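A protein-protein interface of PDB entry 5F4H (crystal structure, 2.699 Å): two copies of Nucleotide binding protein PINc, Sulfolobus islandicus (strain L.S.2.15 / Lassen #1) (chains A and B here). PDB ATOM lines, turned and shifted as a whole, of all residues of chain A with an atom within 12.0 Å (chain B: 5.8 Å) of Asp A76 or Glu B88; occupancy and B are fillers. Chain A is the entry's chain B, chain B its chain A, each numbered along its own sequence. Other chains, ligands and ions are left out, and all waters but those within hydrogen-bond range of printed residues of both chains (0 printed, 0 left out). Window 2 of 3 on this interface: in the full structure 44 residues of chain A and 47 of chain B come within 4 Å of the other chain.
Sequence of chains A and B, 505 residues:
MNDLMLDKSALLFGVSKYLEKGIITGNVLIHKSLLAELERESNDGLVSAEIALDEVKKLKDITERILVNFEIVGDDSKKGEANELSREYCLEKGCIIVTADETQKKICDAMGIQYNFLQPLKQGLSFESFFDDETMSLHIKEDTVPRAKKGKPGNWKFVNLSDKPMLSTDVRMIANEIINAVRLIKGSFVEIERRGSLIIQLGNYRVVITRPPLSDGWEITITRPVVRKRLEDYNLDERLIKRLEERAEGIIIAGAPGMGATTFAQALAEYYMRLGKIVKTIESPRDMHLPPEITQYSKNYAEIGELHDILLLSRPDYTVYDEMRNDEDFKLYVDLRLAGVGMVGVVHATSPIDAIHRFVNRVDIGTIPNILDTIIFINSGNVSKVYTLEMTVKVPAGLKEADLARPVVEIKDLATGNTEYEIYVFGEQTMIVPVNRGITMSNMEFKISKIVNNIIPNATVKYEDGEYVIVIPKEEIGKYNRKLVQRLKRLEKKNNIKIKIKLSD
Of the 12 printed residues of chain B, 5 touch a printed residue of chain A.
Printed residues of chain B that touch a printed residue of chain A: Asn B83, Glu B84, Arg B87, Glu B88 and Leu B91.
Hydrophobic or aromatic side chains of chain B that line the printed part of chain A: Leu B91.
Of the 25 printed residues of chain A, 3 touch a printed residue of chain B.
The side-chain carboxylate (OE1) of Glu A39 is in salt-bridge range of the guanidinium group (NH2) of Arg B87, 2.6 Å away.
The backbone carbonyl oxygen of Val A73 lies within hydrogen-bond range of the backbone NH of Lys A32, 2.8 Å away.
Lys A32 touches Leu B91 (NZ to CD1, 3.9 Å).
Glu A39 touches Asn B83 (OE2 to ND2, 3.8 Å).
OD1 of Asp A76 touches OE2 of Glu B84, at 3.7 Å.
Asp A76 touches Glu B88.
Printed residues of chain B within 4 Å of Lys A32: Leu B91.
Ala A36 touches none of the printed residues of chain B.
Of the printed residues of chain B, Glu A39 touches Asn B83 and Arg B87.
Of the printed residues of chain B, Asp A76 touches Glu B84 and Glu B88.
Ser A77 touches none of the printed residues of chain B.
Of the printed residues of chain A, Asn B83 touches Glu A39 (3.8 Å).
Of chain A, only Asp A76 (3.7 Å) comes within 4 Å of Glu B84.
No residue of chain A comes within 4 Å of Leu B85.
Ser B86 touches none of the printed residues of chain A.
Arg B87 touches one residue of chain A.
Of chain A, only Asp A76 comes within 4 Å of Glu B88.
No residue of chain A comes within 4 Å of Cys B90.
Leu B91 touches one residue of chain A.
The nearest printed residue of chain A that does not touch Asn B83 is Asp A76 (7.3 Å).
Positions printed for both chains: 85, 89 and 93.
Of the 5 pairs that touch across the chains among the printed residues, none has its exchanged pair printed and touching as well.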
ATOM      1  N   ILE A  30      32.887 -20.109  -2.999  1.00  0.00           N
ATOM      2  CA  ILE A  30      31.772 -19.230  -2.704  1.00  0.00           C
ATOM      3  C   ILE A  30      30.912 -19.119  -3.954  1.00  0.00           C
ATOM      4  O   ILE A  30      31.396 -18.909  -5.051  1.00  0.00           O
ATOM      5  CB  ILE A  30      32.262 -17.862  -2.273  1.00  0.00           C
ATOM      6  CG1 ILE A  30      33.028 -17.974  -0.961  1.00  0.00           C
ATOM      7  CG2 ILE A  30      31.108 -16.881  -2.091  1.00  0.00           C
ATOM      8  CD1 ILE A  30      33.532 -16.654  -0.407  1.00  0.00           C
ATOM      9  N   HIS A  31      29.616 -19.207  -3.786  1.00  0.00           N
ATOM     10  CA  HIS A  31      28.753 -19.125  -4.928  1.00  0.00           C
ATOM     11  C   HIS A  31      28.622 -17.695  -5.416  1.00  0.00           C
ATOM     12  O   HIS A  31      28.576 -16.757  -4.626  1.00  0.00           O
ATOM     13  CB  HIS A  31      27.384 -19.656  -4.576  1.00  0.00           C
ATOM     14  CG  HIS A  31      26.615 -20.057  -5.779  1.00  0.00           C
ATOM     15  ND1 HIS A  31      25.932 -19.155  -6.557  1.00  0.00           N
ATOM     16  CD2 HIS A  31      26.477 -21.258  -6.381  1.00  0.00           C
ATOM     17  CE1 HIS A  31      25.401 -19.776  -7.587  1.00  0.00           C
ATOM     18  NE2 HIS A  31      25.700 -21.059  -7.495  1.00  0.00           N
ATOM     19  N   LYS A  32      28.489 -17.534  -6.722  1.00  0.00           N
ATOM     20  CA  LYS A  32      28.360 -16.179  -7.339  1.00  0.00           C
ATOM     21  C   LYS A  32      27.241 -15.361  -6.729  1.00  0.00           C
ATOM     22  O   LYS A  32      27.369 -14.164  -6.458  1.00  0.00           O
ATOM     23  CB  LYS A  32      28.088 -16.271  -8.865  1.00  0.00           C
ATOM     24  CG  LYS A  32      29.228 -15.831  -9.728  1.00  0.00           C
ATOM     25  CD  LYS A  32      28.848 -15.831 -11.197  1.00  0.00           C
ATOM     26  CE  LYS A  32      30.005 -16.214 -12.121  1.00  0.00           C
ATOM     27  NZ  LYS A  32      31.212 -15.364 -11.996  1.00  0.00           N
ATOM     28  N   SER A  33      26.138 -16.048  -6.548  1.00  0.00           N
ATOM     29  CA  SER A  33      24.949 -15.530  -6.019  1.00  0.00           C
ATOM     30  C   SER A  33      25.146 -14.807  -4.700  1.00  0.00           C
ATOM     31  O   SER A  33      24.578 -13.739  -4.449  1.00  0.00           O
ATOM     32  CB  SER A  33      24.016 -16.729  -5.826  1.00  0.00           C
ATOM     33  OG  SER A  33      22.713 -16.275  -5.583  1.00  0.00           O
ATOM     34  N   LEU A  34      25.933 -15.418  -3.837  1.00  0.00           N
ATOM     35  CA  LEU A  34      26.190 -14.854  -2.538  1.00  0.00           C
ATOM     36  C   LEU A  34      26.949 -13.556  -2.687  1.00  0.00           C
ATOM     37  O   LEU A  34      26.665 -12.573  -2.015  1.00  0.00           O
ATOM     38  CB  LEU A  34      26.986 -15.803  -1.676  1.00  0.00           C
ATOM     39  CG  LEU A  34      27.414 -15.244  -0.324  1.00  0.00           C
ATOM     40  CD1 LEU A  34      26.260 -14.725   0.492  1.00  0.00           C
ATOM     41  CD2 LEU A  34      28.101 -16.311   0.481  1.00  0.00           C
ATOM     42  N   LEU A  35      27.909 -13.529  -3.585  1.00  0.00           N
ATOM     43  CA  LEU A  35      28.640 -12.281  -3.831  1.00  0.00           C
ATOM     44  C   LEU A  35      27.783 -11.162  -4.417  1.00  0.00           C
ATOM     45  O   LEU A  35      27.938  -9.982  -4.051  1.00  0.00           O
ATOM     46  CB  LEU A  35      29.793 -12.532  -4.771  1.00  0.00           C
ATOM     47  CG  LEU A  35      31.062 -12.883  -4.040  1.00  0.00           C
ATOM     48  CD1 LEU A  35      32.166 -13.063  -5.051  1.00  0.00           C
ATOM     49  CD2 LEU A  35      31.475 -11.849  -3.011  1.00  0.00           C
ATOM     50  N   ALA A  36      26.856 -11.548  -5.288  1.00  0.00           N
ATOM     51  CA  ALA A  36      25.881 -10.606  -5.819  1.00  0.00           C
ATOM     52  C   ALA A  36      25.051 -10.010  -4.680  1.00  0.00           C
ATOM     53  O   ALA A  36      24.874  -8.817  -4.603  1.00  0.00           O
ATOM     54  CB  ALA A  36      24.976 -11.289  -6.819  1.00  0.00           C
ATOM     55  N   GLU A  37      24.590 -10.870  -3.777  1.00  0.00           N
ATOM     56  CA  GLU A  37      23.767 -10.465  -2.629  1.00  0.00           C
ATOM     57  C   GLU A  37      24.527  -9.504  -1.722  1.00  0.00           C
ATOM     58  O   GLU A  37      24.028  -8.459  -1.371  1.00  0.00           O
ATOM     59  CB  GLU A  37      23.307 -11.704  -1.830  1.00  0.00           C
ATOM     60  CG  GLU A  37      22.387 -11.372  -0.647  1.00  0.00           C
ATOM     61  CD  GLU A  37      22.274 -12.471   0.410  1.00  0.00           C
ATOM     62  OE1 GLU A  37      22.335 -13.687   0.065  1.00  0.00           O
ATOM     63  OE2 GLU A  37      22.113 -12.097   1.605  1.00  0.00           O
ATOM     64  N   LEU A  38      25.750  -9.867  -1.395  1.00  0.00           N
ATOM     65  CA  LEU A  38      26.598  -9.008  -0.583  1.00  0.00           C
ATOM     66  C   LEU A  38      26.823  -7.660  -1.237  1.00  0.00           C
ATOM     67  O   LEU A  38      26.777  -6.627  -0.583  1.00  0.00           O
ATOM     68  CB  LEU A  38      27.927  -9.669  -0.354  1.00  0.00           C
ATOM     69  CG  LEU A  38      27.863 -10.888   0.571  1.00  0.00           C
ATOM     70  CD1 LEU A  38      29.241 -11.504   0.727  1.00  0.00           C
ATOM     71  CD2 LEU A  38      27.284 -10.558   1.938  1.00  0.00           C
ATOM     72  N   GLU A  39      26.982  -7.656  -2.536  1.00  0.00           N
ATOM     73  CA  GLU A  39      27.119  -6.418  -3.217  1.00  0.00           C
ATOM     74  C   GLU A  39      25.894  -5.521  -3.059  1.00  0.00           C
ATOM     75  O   GLU A  39      26.012  -4.343  -2.697  1.00  0.00           O
ATOM     76  CB  GLU A  39      27.399  -6.648  -4.689  1.00  0.00           C
ATOM     77  CG  GLU A  39      27.440  -5.362  -5.498  1.00  0.00           C
ATOM     78  CD  GLU A  39      27.942  -5.612  -6.887  1.00  0.00           C
ATOM     79  OE1 GLU A  39      27.427  -6.576  -7.521  1.00  0.00           O
ATOM     80  OE2 GLU A  39      28.836  -4.853  -7.319  1.00  0.00           O
ATOM     81  N   ARG A  40      24.715  -6.058  -3.334  1.00  0.00           N
ATOM     82  CA  ARG A  40      23.472  -5.239  -3.238  1.00  0.00           C
ATOM     83  C   ARG A  40      23.299  -4.735  -1.803  1.00  0.00           C
ATOM     84  O   ARG A  40      23.019  -3.568  -1.575  1.00  0.00           O
ATOM     85  CB  ARG A  40      22.217  -6.037  -3.610  1.00  0.00           C
ATOM     86  CG  ARG A  40      22.174  -6.629  -5.000  1.00  0.00           C
ATOM     87  CD  ARG A  40      20.880  -7.394  -5.227  1.00  0.00           C
ATOM     88  NE  ARG A  40      20.972  -8.800  -4.910  1.00  0.00           N
ATOM     89  CZ  ARG A  40      21.288  -9.744  -5.792  1.00  0.00           C
ATOM     90  NH1 ARG A  40      21.558  -9.442  -7.076  1.00  0.00           N
ATOM     91  NH2 ARG A  40      21.338 -11.004  -5.374  1.00  0.00           N
ATOM     92  N   ILE A  72      35.144 -18.690  -7.082  1.00  0.00           N
ATOM     93  CA  ILE A  72      33.807 -18.255  -7.102  1.00  0.00           C
ATOM     94  C   ILE A  72      33.148 -19.001  -8.202  1.00  0.00           C
ATOM     95  O   ILE A  72      33.572 -18.956  -9.323  1.00  0.00           O
ATOM     96  CB  ILE A  72      33.719 -16.766  -7.393  1.00  0.00           C
ATOM     97  CG1 ILE A  72      34.683 -15.968  -6.502  1.00  0.00           C
ATOM     98  CG2 ILE A  72      32.259 -16.337  -7.290  1.00  0.00           C
ATOM     99  CD1 ILE A  72      34.440 -16.072  -5.043  1.00  0.00           C
ATOM    100  N   VAL A  73      32.064 -19.675  -7.879  1.00  0.00           N
ATOM    101  CA  VAL A  73      31.444 -20.611  -8.816  1.00  0.00           C
ATOM    102  C   VAL A  73      29.992 -20.300  -9.127  1.00  0.00           C
ATOM    103  O   VAL A  73      29.336 -19.603  -8.370  1.00  0.00           O
ATOM    104  CB  VAL A  73      31.571 -22.038  -8.238  1.00  0.00           C
ATOM    105  CG1 VAL A  73      33.021 -22.379  -7.996  1.00  0.00           C
ATOM    106  CG2 VAL A  73      30.820 -22.187  -6.908  1.00  0.00           C
ATOM    107  N   GLY A  74      29.498 -20.903 -10.190  1.00  0.00           N
ATOM    108  CA  GLY A  74      28.088 -20.870 -10.544  1.00  0.00           C
ATOM    109  C   GLY A  74      27.884 -20.018 -11.779  1.00  0.00           C
ATOM    110  O   GLY A  74      28.699 -19.143 -12.016  1.00  0.00           O
ATOM    111  N   ASP A  75      26.819 -20.266 -12.565  1.00  0.00           N
ATOM    112  CA  ASP A  75      26.597 -19.476 -13.800  1.00  0.00           C
ATOM    113  C   ASP A  75      25.928 -18.167 -13.375  1.00  0.00           C
ATOM    114  O   ASP A  75      25.071 -18.165 -12.481  1.00  0.00           O
ATOM    115  CB  ASP A  75      25.966 -20.234 -15.050  1.00  0.00           C
ATOM    116  CG  ASP A  75      24.475 -20.531 -14.965  1.00  0.00           C
ATOM    117  OD1 ASP A  75      23.725 -19.948 -14.191  1.00  0.00           O
ATOM    118  OD2 ASP A  75      24.038 -21.372 -15.759  1.00  0.00           O
ATOM    119  N   ASP A  76      26.400 -17.056 -13.949  1.00  0.00           N
ATOM    120  CA  ASP A  76      25.783 -15.737 -13.744  1.00  0.00           C
ATOM    121  C   ASP A  76      24.304 -15.784 -14.206  1.00  0.00           C
ATOM    122  O   ASP A  76      23.455 -15.125 -13.600  1.00  0.00           O
ATOM    123  CB  ASP A  76      26.564 -14.644 -14.503  1.00  0.00           C
ATOM    124  CG  ASP A  76      26.616 -13.277 -13.770  1.00  0.00           C
ATOM    125  OD1 ASP A  76      27.030 -13.217 -12.605  1.00  0.00           O
ATOM    126  OD2 ASP A  76      26.284 -12.251 -14.394  1.00  0.00           O
ATOM    127  N   SER A  77      24.021 -16.594 -15.244  1.00  0.00           N
ATOM    128  CA  SER A  77      22.655 -16.819 -15.795  1.00  0.00           C
ATOM    129  C   SER A  77      21.605 -17.304 -14.765  1.00  0.00           C
ATOM    130  O   SER A  77      20.477 -16.791 -14.740  1.00  0.00           O
ATOM    131  CB  SER A  77      22.706 -17.829 -16.956  1.00  0.00           C
ATOM    132  N   LYS A  78      21.990 -18.236 -13.880  1.00  0.00           N
ATOM    133  CA  LYS A  78      21.046 -18.814 -12.878  1.00  0.00           C
ATOM    134  C   LYS A  78      20.702 -17.822 -11.750  1.00  0.00           C
ATOM    135  O   LYS A  78      21.583 -17.130 -11.225  1.00  0.00           O
ATOM    136  CB  LYS A  78      21.504 -20.152 -12.274  1.00  0.00           C
ATOM    137  CG  LYS A  78      20.538 -21.330 -12.279  1.00  0.00           C
ATOM    138  CD  LYS A  78      19.068 -21.016 -12.210  1.00  0.00           C
ATOM    139  CE  LYS A  78      18.220 -22.245 -12.529  1.00  0.00           C
ATOM    140  NZ  LYS A  78      16.799 -21.902 -12.835  1.00  0.00           N
ATOM    141  N   LYS A  79      19.418 -17.789 -11.395  1.00  0.00           N
ATOM    142  CA  LYS A  79      18.870 -16.864 -10.395  1.00  0.00           C
ATOM    143  C   LYS A  79      18.138 -17.628  -9.323  1.00  0.00           C
ATOM    144  O   LYS A  79      17.473 -18.623  -9.613  1.00  0.00           O
ATOM    145  CB  LYS A  79      17.888 -15.836 -11.000  1.00  0.00           C
ATOM    146  CG  LYS A  79      17.023 -15.058  -9.959  1.00  0.00           C
ATOM    147  CD  LYS A  79      16.492 -13.767 -10.582  1.00  0.00           C
ATOM    148  CE  LYS A  79      17.523 -12.649 -10.529  1.00  0.00           C
ATOM    149  NZ  LYS A  79      17.231 -11.695  -9.413  1.00  0.00           N
ATOM    150  N   GLY A  80      18.249 -17.106  -8.101  1.00  0.00           N
ATOM    151  CA  GLY A  80      17.607 -17.679  -6.936  1.00  0.00           C
ATOM    152  C   GLY A  80      18.262 -17.166  -5.654  1.00  0.00           C
ATOM    153  O   GLY A  80      19.117 -16.259  -5.698  1.00  0.00           O
ATOM    154  N   GLU A  81      17.860 -17.750  -4.520  1.00  0.00           N
ATOM    155  CA  GLU A  81      18.471 -17.441  -3.206  1.00  0.00           C
ATOM    156  C   GLU A  81      19.840 -18.070  -3.164  1.00  0.00           C
ATOM    157  O   GLU A  81      20.053 -19.177  -3.653  1.00  0.00           O
ATOM    158  CB  GLU A  81      17.644 -17.956  -2.002  1.00  0.00           C
ATOM    159  CG  GLU A  81      16.749 -16.957  -1.182  1.00  0.00           C
ATOM    160  CD  GLU A  81      16.114 -15.860  -2.020  1.00  0.00           C
ATOM    161  OE1 GLU A  81      16.870 -14.936  -2.419  1.00  0.00           O
ATOM    162  OE2 GLU A  81      14.866 -15.889  -2.237  1.00  0.00           O
ATOM    163  N   ALA A  82      20.790 -17.362  -2.574  1.00  0.00           N
ATOM    164  CA  ALA A  82      22.194 -17.848  -2.518  1.00  0.00           C
ATOM    165  C   ALA A  82      22.333 -19.134  -1.735  1.00  0.00           C
ATOM    166  O   ALA A  82      23.036 -20.071  -2.144  1.00  0.00           O
ATOM    167  CB  ALA A  82      23.094 -16.808  -1.895  1.00  0.00           C
ATOM    168  N   LEU A  85      20.949 -22.067  -3.917  1.00  0.00           N
ATOM    169  CA  LEU A  85      21.897 -22.370  -4.998  1.00  0.00           C
ATOM    170  C   LEU A  85      23.134 -23.036  -4.490  1.00  0.00           C
ATOM    171  O   LEU A  85      23.657 -23.913  -5.154  1.00  0.00           O
ATOM    172  CB  LEU A  85      22.311 -21.107  -5.791  1.00  0.00           C
ATOM    173  CG  LEU A  85      21.243 -20.522  -6.721  1.00  0.00           C
ATOM    174  CD1 LEU A  85      21.827 -19.338  -7.457  1.00  0.00           C
ATOM    175  CD2 LEU A  85      20.687 -21.535  -7.725  1.00  0.00           C
ATOM    176  N   TYR A  89      24.536 -26.708  -5.570  1.00  0.00           N
ATOM    177  CA  TYR A  89      25.896 -26.868  -6.074  1.00  0.00           C
ATOM    178  C   TYR A  89      26.632 -27.969  -5.355  1.00  0.00           C
ATOM    179  O   TYR A  89      27.276 -28.812  -5.976  1.00  0.00           O
ATOM    180  CB  TYR A  89      26.694 -25.572  -5.914  1.00  0.00           C
ATOM    181  CG  TYR A  89      28.013 -25.623  -6.616  1.00  0.00           C
ATOM    182  CD1 TYR A  89      28.111 -25.305  -7.996  1.00  0.00           C
ATOM    183  CD2 TYR A  89      29.161 -25.996  -5.946  1.00  0.00           C
ATOM    184  CE1 TYR A  89      29.325 -25.366  -8.661  1.00  0.00           C
ATOM    185  CE2 TYR A  89      30.375 -26.054  -6.593  1.00  0.00           C
ATOM    186  CZ  TYR A  89      30.456 -25.742  -7.942  1.00  0.00           C
ATOM    187  OH  TYR A  89      31.671 -25.805  -8.559  1.00  0.00           O
ATOM    188  N   LYS A  93      28.069 -31.417  -7.062  1.00  0.00           N
ATOM    189  CA  LYS A  93      29.529 -31.566  -7.123  1.00  0.00           C
ATOM    190  C   LYS A  93      30.180 -32.185  -5.872  1.00  0.00           C
ATOM    191  O   LYS A  93      31.376 -32.357  -5.809  1.00  0.00           O
ATOM    192  CB  LYS A  93      30.107 -30.208  -7.485  1.00  0.00           C
ATOM    193  CG  LYS A  93      29.427 -29.600  -8.722  1.00  0.00           C
ATOM    194  CD  LYS A  93      30.208 -29.453 -10.012  1.00  0.00           C
ATOM    195  CE  LYS A  93      29.323 -28.748 -11.040  1.00  0.00           C
ATOM    196  NZ  LYS A  93      30.082 -28.325 -12.256  1.00  0.00           N
ATOM    197  N   ASN B  83      27.061  -3.274 -12.919  1.00  0.00           N
ATOM    198  CA  ASN B  83      28.317  -3.853 -12.456  1.00  0.00           C
ATOM    199  C   ASN B  83      28.441  -5.367 -12.704  1.00  0.00           C
ATOM    200  O   ASN B  83      29.469  -5.856 -13.079  1.00  0.00           O
ATOM    201  CB  ASN B  83      28.535  -3.527 -10.996  1.00  0.00           C
ATOM    202  CG  ASN B  83      29.262  -2.231 -10.821  1.00  0.00           C
ATOM    203  OD1 ASN B  83      29.395  -1.440 -11.723  1.00  0.00           O
ATOM    204  ND2 ASN B  83      29.729  -2.016  -9.650  1.00  0.00           N
ATOM    205  N   GLU B  84      27.358  -6.079 -12.428  1.00  0.00           N
ATOM    206  CA  GLU B  84      27.347  -7.521 -12.557  1.00  0.00           C
ATOM    207  C   GLU B  84      27.580  -7.923 -13.994  1.00  0.00           C
ATOM    208  O   GLU B  84      28.403  -8.790 -14.261  1.00  0.00           O
ATOM    209  CB  GLU B  84      26.017  -8.053 -12.104  1.00  0.00           C
ATOM    210  CG  GLU B  84      26.038  -9.465 -11.581  1.00  0.00           C
ATOM    211  CD  GLU B  84      24.679  -9.858 -10.993  1.00  0.00           C
ATOM    212  OE1 GLU B  84      23.886  -8.971 -10.519  1.00  0.00           O
ATOM    213  OE2 GLU B  84      24.435 -11.082 -11.018  1.00  0.00           O
ATOM    214  N   LEU B  85      26.864  -7.258 -14.891  1.00  0.00           N
ATOM    215  CA  LEU B  85      26.982  -7.509 -16.302  1.00  0.00           C
ATOM    216  C   LEU B  85      28.356  -7.113 -16.815  1.00  0.00           C
ATOM    217  O   LEU B  85      28.910  -7.814 -17.677  1.00  0.00           O
ATOM    218  CB  LEU B  85      25.933  -6.733 -17.100  1.00  0.00           C
ATOM    219  CG  LEU B  85      24.473  -7.136 -16.908  1.00  0.00           C
ATOM    220  CD1 LEU B  85      23.613  -6.376 -17.899  1.00  0.00           C
ATOM    221  CD2 LEU B  85      24.233  -8.631 -17.042  1.00  0.00           C
ATOM    222  N   SER B  86      28.875  -5.977 -16.317  1.00  0.00           N
ATOM    223  CA  SER B  86      30.163  -5.448 -16.765  1.00  0.00           C
ATOM    224  C   SER B  86      31.241  -6.441 -16.363  1.00  0.00           C
ATOM    225  O   SER B  86      32.128  -6.756 -17.163  1.00  0.00           O
ATOM    226  CB  SER B  86      30.488  -4.123 -16.121  1.00  0.00           C
ATOM    227  OG  SER B  86      29.673  -3.042 -16.503  1.00  0.00           O
ATOM    228  N   ARG B  87      31.141  -6.997 -15.161  1.00  0.00           N
ATOM    229  CA  ARG B  87      32.114  -8.005 -14.711  1.00  0.00           C
ATOM    230  C   ARG B  87      32.085  -9.255 -15.546  1.00  0.00           C
ATOM    231  O   ARG B  87      33.117  -9.855 -15.831  1.00  0.00           O
ATOM    232  CB  ARG B  87      31.860  -8.415 -13.277  1.00  0.00           C
ATOM    233  CG  ARG B  87      32.349  -7.411 -12.277  1.00  0.00           C
ATOM    234  CD  ARG B  87      32.249  -7.936 -10.870  1.00  0.00           C
ATOM    235  NE  ARG B  87      30.894  -8.126 -10.378  1.00  0.00           N
ATOM    236  CZ  ARG B  87      30.261  -7.353  -9.535  1.00  0.00           C
ATOM    237  NH1 ARG B  87      30.778  -6.216  -9.120  1.00  0.00           N
ATOM    238  NH2 ARG B  87      29.070  -7.716  -9.140  1.00  0.00           N
ATOM    239  N   GLU B  88      30.878  -9.678 -15.890  1.00  0.00           N
ATOM    240  CA  GLU B  88      30.706 -10.901 -16.665  1.00  0.00           C
ATOM    241  C   GLU B  88      31.354 -10.729 -18.006  1.00  0.00           C
ATOM    242  O   GLU B  88      32.051 -11.602 -18.467  1.00  0.00           O
ATOM    243  CB  GLU B  88      29.227 -11.287 -16.843  1.00  0.00           C
ATOM    244  CG  GLU B  88      28.883 -12.695 -16.304  1.00  0.00           C
ATOM    245  CD  GLU B  88      29.670 -13.882 -16.925  1.00  0.00           C
ATOM    246  OE1 GLU B  88      29.880 -13.960 -18.167  1.00  0.00           O
ATOM    247  OE2 GLU B  88      30.092 -14.777 -16.143  1.00  0.00           O
ATOM    248  N   TYR B  89      31.133  -9.563 -18.596  1.00  0.00           N
ATOM    249  CA  TYR B  89      31.721  -9.235 -19.909  1.00  0.00           C
ATOM    250  C   TYR B  89      33.237  -9.328 -19.835  1.00  0.00           C
ATOM    251  O   TYR B  89      33.858  -9.885 -20.714  1.00  0.00           O
ATOM    252  CB  TYR B  89      31.330  -7.831 -20.361  1.00  0.00           C
ATOM    253  CG  TYR B  89      31.725  -7.499 -21.786  1.00  0.00           C
ATOM    254  CD1 TYR B  89      33.027  -7.050 -22.101  1.00  0.00           C
ATOM    255  CD2 TYR B  89      30.804  -7.574 -22.823  1.00  0.00           C
ATOM    256  CE1 TYR B  89      33.360  -6.703 -23.407  1.00  0.00           C
ATOM    257  CE2 TYR B  89      31.121  -7.241 -24.124  1.00  0.00           C
ATOM    258  CZ  TYR B  89      32.391  -6.816 -24.414  1.00  0.00           C
ATOM    259  OH  TYR B  89      32.673  -6.493 -25.708  1.00  0.00           O
ATOM    260  N   CYS B  90      33.807  -8.796 -18.762  1.00  0.00           N
ATOM    261  CA  CYS B  90      35.249  -8.819 -18.571  1.00  0.00           C
ATOM    262  C   CYS B  90      35.768 -10.236 -18.436  1.00  0.00           C
ATOM    263  O   CYS B  90      36.811 -10.561 -18.987  1.00  0.00           O
ATOM    264  CB  CYS B  90      35.660  -8.008 -17.348  1.00  0.00           C
ATOM    265  SG  CYS B  90      35.350  -6.234 -17.538  1.00  0.00           S
ATOM    266  N   LEU B  91      35.042 -11.071 -17.724  1.00  0.00           N
ATOM    267  CA  LEU B  91      35.428 -12.468 -17.599  1.00  0.00           C
ATOM    268  C   LEU B  91      35.418 -13.227 -18.899  1.00  0.00           C
ATOM    269  O   LEU B  91      36.361 -13.916 -19.241  1.00  0.00           O
ATOM    270  CB  LEU B  91      34.463 -13.187 -16.692  1.00  0.00           C
ATOM    271  CG  LEU B  91      34.900 -13.375 -15.268  1.00  0.00           C
ATOM    272  CD1 LEU B  91      33.945 -14.311 -14.551  1.00  0.00           C
ATOM    273  CD2 LEU B  91      36.316 -13.898 -15.176  1.00  0.00           C
ATOM    274  N   GLU B  92      34.347 -13.044 -19.635  1.00  0.00           N
ATOM    275  CA  GLU B  92      34.151 -13.657 -20.916  1.00  0.00           C
ATOM    276  C   GLU B  92      35.193 -13.149 -21.942  1.00  0.00           C
ATOM    277  O   GLU B  92      35.803 -13.927 -22.642  1.00  0.00           O
ATOM    278  CB  GLU B  92      32.689 -13.300 -21.374  1.00  0.00           C
ATOM    279  CG  GLU B  92      32.192 -13.943 -22.664  1.00  0.00           C
ATOM    280  CD  GLU B  92      30.797 -13.464 -23.097  1.00  0.00           C
ATOM    281  OE1 GLU B  92      30.115 -12.706 -22.356  1.00  0.00           O
ATOM    282  OE2 GLU B  92      30.362 -13.871 -24.199  1.00  0.00           O
ATOM    283  N   LYS B  93      35.426 -11.856 -22.002  1.00  0.00           N
ATOM    284  CA  LYS B  93      36.304 -11.262 -23.022  1.00  0.00           C
ATOM    285  C   LYS B  93      37.721 -10.788 -22.552  1.00  0.00           C
ATOM    286  O   LYS B  93      38.510 -10.302 -23.347  1.00  0.00           O
ATOM    287  CB  LYS B  93      35.562 -10.121 -23.677  1.00  0.00           C
ATOM    288  CG  LYS B  93      34.267 -10.540 -24.297  1.00  0.00           C
ATOM    289  CD  LYS B  93      34.219 -10.198 -25.764  1.00  0.00           C
ATOM    290  CE  LYS B  93      33.426 -11.221 -26.585  1.00  0.00           C
ATOM    291  NZ  LYS B  93      33.250 -10.792 -28.013  1.00  0.00           N
ATOM    292  N   ILE B 113      39.169 -11.193 -11.743  1.00  0.00           N
ATOM    293  CA  ILE B 113      39.085 -10.248 -12.805  1.00  0.00           C
ATOM    294  C   ILE B 113      40.161  -9.188 -12.628  1.00  0.00           C
ATOM    295  O   ILE B 113      40.267  -8.613 -11.565  1.00  0.00           O
ATOM    296  CB  ILE B 113      37.725  -9.561 -12.814  1.00  0.00           C
ATOM    297  CG1 ILE B 113      36.646 -10.629 -12.896  1.00  0.00           C
ATOM    298  CG2 ILE B 113      37.620  -8.594 -14.002  1.00  0.00           C
ATOM    299  CD1 ILE B 113      35.229 -10.101 -13.063  1.00  0.00           C
